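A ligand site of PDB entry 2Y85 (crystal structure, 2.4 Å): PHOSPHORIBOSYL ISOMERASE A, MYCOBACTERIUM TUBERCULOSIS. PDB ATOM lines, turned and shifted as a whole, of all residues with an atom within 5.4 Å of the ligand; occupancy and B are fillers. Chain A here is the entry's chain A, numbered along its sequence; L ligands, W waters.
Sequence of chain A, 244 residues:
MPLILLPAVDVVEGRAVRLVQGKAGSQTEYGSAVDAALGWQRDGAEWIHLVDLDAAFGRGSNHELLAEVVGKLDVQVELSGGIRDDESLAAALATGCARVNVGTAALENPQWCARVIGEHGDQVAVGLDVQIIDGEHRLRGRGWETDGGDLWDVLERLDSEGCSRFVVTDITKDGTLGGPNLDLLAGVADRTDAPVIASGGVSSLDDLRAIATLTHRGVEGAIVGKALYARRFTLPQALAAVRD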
ATOM      1  N   ALA A   8     -18.421  23.256   4.754  1.00  0.00           N
ATOM      2  CA  ALA A   8     -17.727  21.975   4.598  1.00  0.00           C
ATOM      3  C   ALA A   8     -17.740  21.534   3.143  1.00  0.00           C
ATOM      4  O   ALA A   8     -18.769  21.554   2.466  1.00  0.00           O
ATOM      5  CB  ALA A   8     -18.360  20.910   5.491  1.00  0.00           C
ATOM      6  N   ASP A  10     -16.519  18.145   1.386  1.00  0.00           N
ATOM      7  CA  ASP A  10     -16.069  16.768   1.568  1.00  0.00           C
ATOM      8  C   ASP A  10     -15.724  16.163   0.215  1.00  0.00           C
ATOM      9  O   ASP A  10     -16.559  16.135  -0.701  1.00  0.00           O
ATOM     10  CB  ASP A  10     -17.161  15.926   2.219  1.00  0.00           C
ATOM     11  CG  ASP A  10     -17.400  16.287   3.681  1.00  0.00           C
ATOM     12  OD1 ASP A  10     -16.705  17.144   4.262  1.00  0.00           O
ATOM     13  OD2 ASP A  10     -18.339  15.673   4.252  1.00  0.00           O
ATOM     14  N   HIS A  49     -13.891  24.291   5.702  1.00  0.00           N
ATOM     15  CA  HIS A  49     -13.554  22.974   6.239  1.00  0.00           C
ATOM     16  C   HIS A  49     -13.415  22.001   5.050  1.00  0.00           C
ATOM     17  O   HIS A  49     -14.396  21.644   4.430  1.00  0.00           O
ATOM     18  CB  HIS A  49     -14.648  22.514   7.195  1.00  0.00           C
ATOM     19  CG  HIS A  49     -14.294  21.303   8.003  1.00  0.00           C
ATOM     20  ND1 HIS A  49     -13.267  21.305   8.915  1.00  0.00           N
ATOM     21  CD2 HIS A  49     -14.837  20.065   8.035  1.00  0.00           C
ATOM     22  CE1 HIS A  49     -13.182  20.111   9.479  1.00  0.00           C
ATOM     23  NE2 HIS A  49     -14.123  19.339   8.973  1.00  0.00           N
ATOM     24  N   VAL A  51     -12.258  18.365   3.509  1.00  0.00           N
ATOM     25  CA  VAL A  51     -12.186  16.990   4.013  1.00  0.00           C
ATOM     26  C   VAL A  51     -11.880  15.961   2.928  1.00  0.00           C
ATOM     27  O   VAL A  51     -12.564  15.863   1.908  1.00  0.00           O
ATOM     28  CB  VAL A  51     -13.506  16.578   4.751  1.00  0.00           C
ATOM     29  CG1 VAL A  51     -13.335  15.251   5.530  1.00  0.00           C
ATOM     30  CG2 VAL A  51     -13.986  17.707   5.692  1.00  0.00           C
ATOM     31  N   LEU A  53     -12.390  12.493   2.523  1.00  0.00           N
ATOM     32  CA  LEU A  53     -13.137  11.352   3.070  1.00  0.00           C
ATOM     33  C   LEU A  53     -12.420  10.056   2.810  1.00  0.00           C
ATOM     34  O   LEU A  53     -12.373   9.189   3.680  1.00  0.00           O
ATOM     35  CB  LEU A  53     -14.560  11.277   2.508  1.00  0.00           C
ATOM     36  CG  LEU A  53     -15.533  12.305   3.111  1.00  0.00           C
ATOM     37  CD1 LEU A  53     -16.886  12.227   2.412  1.00  0.00           C
ATOM     38  CD2 LEU A  53     -15.715  12.066   4.599  1.00  0.00           C
ATOM     39  N   ALA A  56      -9.843   9.615   5.294  1.00  0.00           N
ATOM     40  CA  ALA A  56     -10.427   9.358   6.614  1.00  0.00           C
ATOM     41  C   ALA A  56     -10.804   7.893   6.816  1.00  0.00           C
ATOM     42  O   ALA A  56     -10.602   7.347   7.906  1.00  0.00           O
ATOM     43  CB  ALA A  56     -11.637  10.266   6.848  1.00  0.00           C
ATOM     44  N   PHE A  57     -11.340   7.260   5.768  1.00  0.00           N
ATOM     45  CA  PHE A  57     -11.681   5.843   5.785  1.00  0.00           C
ATOM     46  C   PHE A  57     -10.512   4.936   5.423  1.00  0.00           C
ATOM     47  O   PHE A  57     -10.648   3.712   5.427  1.00  0.00           O
ATOM     48  CB  PHE A  57     -12.856   5.582   4.830  1.00  0.00           C
ATOM     49  CG  PHE A  57     -14.191   6.023   5.387  1.00  0.00           C
ATOM     50  CD1 PHE A  57     -14.511   7.381   5.469  1.00  0.00           C
ATOM     51  CD2 PHE A  57     -15.098   5.079   5.878  1.00  0.00           C
ATOM     52  CE1 PHE A  57     -15.724   7.791   5.999  1.00  0.00           C
ATOM     53  CE2 PHE A  57     -16.320   5.491   6.405  1.00  0.00           C
ATOM     54  CZ  PHE A  57     -16.635   6.834   6.461  1.00  0.00           C
ATOM     55  N   SER A  80      -8.832  18.488   6.911  1.00  0.00           N
ATOM     56  CA  SER A  80      -9.236  17.375   7.739  1.00  0.00           C
ATOM     57  C   SER A  80      -9.337  16.102   6.915  1.00  0.00           C
ATOM     58  O   SER A  80      -9.559  16.174   5.702  1.00  0.00           O
ATOM     59  CB  SER A  80     -10.578  17.679   8.400  1.00  0.00           C
ATOM     60  OG  SER A  80     -10.768  16.894   9.561  1.00  0.00           O
ATOM     61  N   GLY A  81      -9.141  14.954   7.570  1.00  0.00           N
ATOM     62  CA  GLY A  81      -9.316  13.662   6.907  1.00  0.00           C
ATOM     63  C   GLY A  81      -8.079  12.788   6.955  1.00  0.00           C
ATOM     64  O   GLY A  81      -7.127  13.034   6.215  1.00  0.00           O
ATOM     65  N   ASN A 101      -6.851  19.359  11.149  1.00  0.00           N
ATOM     66  CA  ASN A 101      -7.756  18.783  12.107  1.00  0.00           C
ATOM     67  C   ASN A 101      -7.266  17.350  12.260  1.00  0.00           C
ATOM     68  O   ASN A 101      -7.347  16.546  11.315  1.00  0.00           O
ATOM     69  CB  ASN A 101      -9.186  18.890  11.542  1.00  0.00           C
ATOM     70  CG  ASN A 101     -10.265  18.643  12.575  1.00  0.00           C
ATOM     71  OD1 ASN A 101     -10.018  18.666  13.785  1.00  0.00           O
ATOM     72  ND2 ASN A 101     -11.501  18.433  12.098  1.00  0.00           N
ATOM     73  N   ASP A 129     -14.889  12.803  17.926  1.00  0.00           N
ATOM     74  CA  ASP A 129     -16.061  12.145  17.351  1.00  0.00           C
ATOM     75  C   ASP A 129     -16.693  11.273  18.436  1.00  0.00           C
ATOM     76  O   ASP A 129     -16.120  10.247  18.825  1.00  0.00           O
ATOM     77  CB  ASP A 129     -15.641  11.258  16.170  1.00  0.00           C
ATOM     78  CG  ASP A 129     -15.201  12.053  14.960  1.00  0.00           C
ATOM     79  OD1 ASP A 129     -14.964  13.280  15.070  1.00  0.00           O
ATOM     80  OD2 ASP A 129     -15.092  11.429  13.888  1.00  0.00           O
ATOM     81  N   ARG A 142     -15.196   8.750  12.967  1.00  0.00           N
ATOM     82  CA  ARG A 142     -15.814   8.535  11.652  1.00  0.00           C
ATOM     83  C   ARG A 142     -14.739   8.008  10.725  1.00  0.00           C
ATOM     84  O   ARG A 142     -13.616   8.542  10.678  1.00  0.00           O
ATOM     85  CB  ARG A 142     -16.406   9.824  11.103  1.00  0.00           C
ATOM     86  CG  ARG A 142     -17.571  10.359  11.923  1.00  0.00           C
ATOM     87  CD  ARG A 142     -17.917  11.748  11.520  1.00  0.00           C
ATOM     88  NE  ARG A 142     -16.956  12.681  12.052  1.00  0.00           N
ATOM     89  CZ  ARG A 142     -16.924  13.969  11.776  1.00  0.00           C
ATOM     90  NH1 ARG A 142     -17.816  14.509  10.959  1.00  0.00           N
ATOM     91  NH2 ARG A 142     -16.005  14.728  12.333  1.00  0.00           N
ATOM     92  N   GLY A 143     -15.051   6.935  10.022  1.00  0.00           N
ATOM     93  CA  GLY A 143     -14.065   6.339   9.141  1.00  0.00           C
ATOM     94  C   GLY A 143     -13.092   5.387   9.806  1.00  0.00           C
ATOM     95  O   GLY A 143     -12.333   4.718   9.110  1.00  0.00           O
ATOM     96  N   THR A 169     -17.833  16.399  17.424  1.00  0.00           N
ATOM     97  CA  THR A 169     -18.935  15.843  16.637  1.00  0.00           C
ATOM     98  C   THR A 169     -19.675  14.755  17.414  1.00  0.00           C
ATOM     99  O   THR A 169     -19.045  13.936  18.094  1.00  0.00           O
ATOM    100  CB  THR A 169     -18.450  15.212  15.304  1.00  0.00           C
ATOM    101  OG1 THR A 169     -17.728  16.176  14.550  1.00  0.00           O
ATOM    102  CG2 THR A 169     -19.616  14.705  14.487  1.00  0.00           C
ATOM    103  N   LYS A 173     -25.516  12.600  14.835  1.00  0.00           N
ATOM    104  CA  LYS A 173     -26.193  13.772  14.290  1.00  0.00           C
ATOM    105  C   LYS A 173     -25.538  14.265  12.998  1.00  0.00           C
ATOM    106  O   LYS A 173     -26.157  14.999  12.229  1.00  0.00           O
ATOM    107  CB  LYS A 173     -26.174  14.918  15.314  1.00  0.00           C
ATOM    108  CG  LYS A 173     -26.731  14.576  16.679  1.00  0.00           C
ATOM    109  CD  LYS A 173     -28.175  14.077  16.638  1.00  0.00           C
ATOM    110  CE  LYS A 173     -29.011  14.626  17.768  1.00  0.00           C
ATOM    111  NZ  LYS A 173     -29.548  15.998  17.429  1.00  0.00           N
ATOM    112  N   ASP A 174     -24.290  13.860  12.768  1.00  0.00           N
ATOM    113  CA  ASP A 174     -23.530  14.261  11.576  1.00  0.00           C
ATOM    114  C   ASP A 174     -24.230  13.887  10.256  1.00  0.00           C
ATOM    115  O   ASP A 174     -24.488  12.712   9.968  1.00  0.00           O
ATOM    116  CB  ASP A 174     -22.125  13.617  11.652  1.00  0.00           C
ATOM    117  CG  ASP A 174     -21.176  14.137  10.594  1.00  0.00           C
ATOM    118  OD1 ASP A 174     -21.196  15.342  10.250  1.00  0.00           O
ATOM    119  OD2 ASP A 174     -20.355  13.318  10.107  1.00  0.00           O
ATOM    120  N   GLY A 175     -24.551  14.914   9.470  1.00  0.00           N
ATOM    121  CA  GLY A 175     -25.169  14.750   8.160  1.00  0.00           C
ATOM    122  C   GLY A 175     -26.638  14.400   8.203  1.00  0.00           C
ATOM    123  O   GLY A 175     -27.196  14.003   7.199  1.00  0.00           O
ATOM    124  N   THR A 176     -27.275  14.562   9.356  1.00  0.00           N
ATOM    125  CA  THR A 176     -28.644  14.076   9.572  1.00  0.00           C
ATOM    126  C   THR A 176     -29.731  15.142   9.513  1.00  0.00           C
ATOM    127  O   THR A 176     -30.912  14.794   9.425  1.00  0.00           O
ATOM    128  CB  THR A 176     -28.790  13.395  10.953  1.00  0.00           C
ATOM    129  OG1 THR A 176     -28.524  14.350  11.977  1.00  0.00           O
ATOM    130  CG2 THR A 176     -27.842  12.234  11.087  1.00  0.00           C
ATOM    131  N   LEU A 177     -29.348  16.420   9.588  1.00  0.00           N
ATOM    132  CA  LEU A 177     -30.282  17.549   9.665  1.00  0.00           C
ATOM    133  C   LEU A 177     -31.260  17.369  10.798  1.00  0.00           C
ATOM    134  O   LEU A 177     -32.428  17.700  10.663  1.00  0.00           O
ATOM    135  CB  LEU A 177     -31.074  17.738   8.358  1.00  0.00           C
ATOM    136  CG  LEU A 177     -30.272  18.023   7.090  1.00  0.00           C
ATOM    137  CD1 LEU A 177     -31.170  17.882   5.874  1.00  0.00           C
ATOM    138  CD2 LEU A 177     -29.644  19.405   7.131  1.00  0.00           C
ATOM    139  N   SER A 199     -19.482  20.467  14.995  1.00  0.00           N
ATOM    140  CA  SER A 199     -19.649  19.857  13.668  1.00  0.00           C
ATOM    141  C   SER A 199     -20.763  18.836  13.711  1.00  0.00           C
ATOM    142  O   SER A 199     -20.808  18.002  14.614  1.00  0.00           O
ATOM    143  CB  SER A 199     -18.350  19.162  13.243  1.00  0.00           C
ATOM    144  OG  SER A 199     -18.399  18.744  11.873  1.00  0.00           O
ATOM    145  N   GLY A 200     -21.692  18.901  12.756  1.00  0.00           N
ATOM    146  CA  GLY A 200     -22.731  17.890  12.597  1.00  0.00           C
ATOM    147  C   GLY A 200     -24.142  18.286  12.999  1.00  0.00           C
ATOM    148  O   GLY A 200     -24.376  18.766  14.107  1.00  0.00           O
ATOM    149  N   GLY A 201     -25.088  18.078  12.084  1.00  0.00           N
ATOM    150  CA  GLY A 201     -26.508  18.070  12.442  1.00  0.00           C
ATOM    151  C   GLY A 201     -27.271  19.378  12.354  1.00  0.00           C
ATOM    152  O   GLY A 201     -28.460  19.404  12.668  1.00  0.00           O
ATOM    153  N   VAL A 202     -26.612  20.463  11.951  1.00  0.00           N
ATOM    154  CA  VAL A 202     -27.333  21.728  11.744  1.00  0.00           C
ATOM    155  C   VAL A 202     -28.348  21.520  10.626  1.00  0.00           C
ATOM    156  O   VAL A 202     -28.019  21.025   9.547  1.00  0.00           O
ATOM    157  CB  VAL A 202     -26.409  22.926  11.413  1.00  0.00           C
ATOM    158  CG1 VAL A 202     -27.217  24.117  10.912  1.00  0.00           C
ATOM    159  CG2 VAL A 202     -25.618  23.343  12.632  1.00  0.00           C
ATOM    160  N   ILE A 223     -19.324  24.159  12.046  1.00  0.00           N
ATOM    161  CA  ILE A 223     -19.157  23.617  10.689  1.00  0.00           C
ATOM    162  C   ILE A 223     -20.497  23.185  10.133  1.00  0.00           C
ATOM    163  O   ILE A 223     -21.255  22.517  10.799  1.00  0.00           O
ATOM    164  CB  ILE A 223     -18.165  22.404  10.663  1.00  0.00           C
ATOM    165  CG1 ILE A 223     -16.735  22.851  11.039  1.00  0.00           C
ATOM    166  CG2 ILE A 223     -18.153  21.722   9.274  1.00  0.00           C
ATOM    167  CD1 ILE A 223     -15.907  21.793  11.702  1.00  0.00           C
ATOM    168  N   VAL A 224     -20.800  23.591   8.893  1.00  0.00           N
ATOM    169  CA  VAL A 224     -22.096  23.324   8.272  1.00  0.00           C
ATOM    170  C   VAL A 224     -21.915  22.760   6.859  1.00  0.00           C
ATOM    171  O   VAL A 224     -21.345  23.412   5.975  1.00  0.00           O
ATOM    172  CB  VAL A 224     -22.947  24.617   8.174  1.00  0.00           C
ATOM    173  CG1 VAL A 224     -24.326  24.338   7.530  1.00  0.00           C
ATOM    174  CG2 VAL A 224     -23.110  25.255   9.557  1.00  0.00           C
ATOM    175  N   GLY A 225     -22.412  21.539   6.655  1.00  0.00           N
ATOM    176  CA  GLY A 225     -22.378  20.888   5.347  1.00  0.00           C
ATOM    177  C   GLY A 225     -23.737  20.779   4.677  1.00  0.00           C
ATOM    178  O   GLY A 225     -24.050  21.514   3.723  1.00  0.00           O
ATOM    179  N   LYS A 226     -24.534  19.853   5.180  1.00  0.00           N
ATOM    180  CA  LYS A 226     -25.754  19.401   4.519  1.00  0.00           C
ATOM    181  C   LYS A 226     -26.859  20.481   4.401  1.00  0.00           C
ATOM    182  O   LYS A 226     -27.527  20.596   3.364  1.00  0.00           O
ATOM    183  CB  LYS A 226     -26.272  18.187   5.288  1.00  0.00           C
ATOM    184  CG  LYS A 226     -27.397  17.429   4.605  1.00  0.00           C
ATOM    185  CD  LYS A 226     -27.590  16.093   5.266  1.00  0.00           C
ATOM    186  CE  LYS A 226     -28.718  15.281   4.615  1.00  0.00           C
ATOM    187  NZ  LYS A 226     -28.303  14.699   3.298  1.00  0.00           N
ATOM    188  N   ALA A 227     -27.052  21.265   5.454  1.00  0.00           N
ATOM    189  CA  ALA A 227     -28.074  22.320   5.451  1.00  0.00           C
ATOM    190  C   ALA A 227     -27.823  23.407   4.394  1.00  0.00           C
ATOM    191  O   ALA A 227     -28.759  24.086   3.982  1.00  0.00           O
ATOM    192  CB  ALA A 227     -28.178  22.934   6.838  1.00  0.00           C
HETATM  193  P1  LIG L   1     -23.404  18.299   8.474  1.00  0.00           P
HETATM  194  O1  LIG L   1     -24.509  17.625   9.401  1.00  0.00           O
HETATM  195  O2  LIG L   1     -23.701  19.844   8.471  1.00  0.00           O
HETATM  196  O3  LIG L   1     -23.327  17.715   7.122  1.00  0.00           O
HETATM  197  O4  LIG L   1     -22.026  18.144   9.210  1.00  0.00           O
HETATM  198  C1  LIG L   1     -20.911  18.847   8.610  1.00  0.00           C
HETATM  199  C2  LIG L   1     -19.589  18.109   8.760  1.00  0.00           C
HETATM  200  O5  LIG L   1     -19.481  17.507  10.041  1.00  0.00           O
HETATM  201  C3  LIG L   1     -19.406  17.027   7.705  1.00  0.00           C
HETATM  202  O6  LIG L   1     -19.866  17.533   6.455  1.00  0.00           O
HETATM  203  C4  LIG L   1     -17.890  16.711   7.643  1.00  0.00           C
HETATM  204  O7  LIG L   1     -17.140  17.737   6.917  1.00  0.00           O
HETATM  205  C5  LIG L   1     -17.499  15.295   7.174  1.00  0.00           C
HETATM  206  N1  LIG L   1     -16.508  14.905   8.182  1.00  0.00           N
HETATM  207  C6  LIG L   1     -14.520  13.763   8.748  1.00  0.00           C
HETATM  208  C7  LIG L   1     -15.849  13.770   8.287  1.00  0.00           C
HETATM  209  C8  LIG L   1     -16.485  12.566   7.996  1.00  0.00           C
HETATM  210  C9  LIG L   1     -15.796  11.360   8.150  1.00  0.00           C
HETATM  211  C10 LIG L   1     -14.474  11.349   8.599  1.00  0.00           C
HETATM  212  C11 LIG L   1     -13.842  12.545   8.894  1.00  0.00           C
HETATM  213  C12 LIG L   1     -13.767  15.071   9.060  1.00  0.00           C
HETATM  214  O8  LIG L   1     -12.601  15.022   9.488  1.00  0.00           O
HETATM  215  O9  LIG L   1     -14.330  16.150   8.832  1.00  0.00           O
HETATM  216  O   HOH W   1     -15.981  17.446  10.835  1.00  0.00           O
HETATM  217  O   HOH W   2     -27.020  18.058   9.337  1.00  0.00           O
HETATM  218  O   HOH W   3     -11.130  13.441  10.787  1.00  0.00           O
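OG of Ser 199 sits at hydrogen-bond distance from O5 of the ligand (2.5 Å). OG of Ser 80 lies within hydrogen-bond range of O8 of the ligand (2.6 Å). N of Gly 175 lies within hydrogen-bond range of O1 of the ligand, 2.7 Å away. An oxygen (O7) of the ligand lies within hydrogen-bond range of the side-chain carboxylate (OD1) of Asp 10 (2.8 Å). An oxygen (O5) of the ligand is in hydrogen-bond range of the side-chain carboxylate of Asp 174, at 2.8 Å. An oxygen (O1) of the ligand is in hydrogen-bond range of the backbone NH (N) of Gly 201, 2.8 Å away. The backbone NH (N) of Gly 225 is in hydrogen-bond range of an oxygen (O2) of the ligand. The backbone NH (N) of Lys 226 sits at hydrogen-bond distance from an oxygen (O3) of the ligand (3.1 Å). An oxygen (O9) of the ligand is in hydrogen-bond range of a ring nitrogen (NE2) of His 49.
ND2 of Asn 101 sits at hydrogen-bond distance from OG of Ser 80 (3.1 Å). The guanidinium group (NH1) of Arg 142 lies within salt-bridge range of the side-chain carboxylate (OD2) of Asp 174 (2.9 Å). The backbone NH (N) of Gly 201 lies close to the backbone carbonyl oxygen (O) of Lys 173 (3.3 Å). OG1 of Thr 169 lies within hydrogen-bond range of NH2 of Arg 142 (3.2 Å). The guanidinium group (NE) of Arg 142 lies within salt-bridge range of the side-chain carboxylate (OD2) of Asp 129. O of Val 224 sits at hydrogen-bond distance from N of Ala 8 (3.2 Å).
The guanidinium group (NH1) of Arg 142 lies close to a nitrogen (N1) of the ligand, at 3.1 Å. Residues that only touch the ligand: Ala 8 (3.7 Å), Val 51 (3.4 Å), Leu 53 (3.5 Å), Ala 56 (3.5 Å), Gly 81 (3.96 Å), Gly 200 (3.5 Å), Ile 223 (3.9 Å) and Val 224 (3.8 Å). Hydrophobic or aromatic side chains that line the ligand: Ala 8, His 49, Val 51, Leu 53, Ala 56 and Ile 223. Within 4 Å of the ligand: Ala 8, Asp 10, His 49, Val 51, Leu 53, Ala 56, Ser 80, Gly 81, Arg 142, Asp 174, Gly 175, Ser 199, Gly 200, Gly 201, Ile 223, Val 224, Gly 225 and Lys 226.
Water W2 lies within hydrogen-bond range of O1 of the ligand (2.5 Å), N of Leu 177 (2.9 Å), O of Val 202 (3.1 Å) and N of Gly 201 (3.4 Å). Water W1 lies within hydrogen-bond range of O9 of the ligand, OG of Ser 199, NH2 of Arg 142 and NE2 of His 49.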
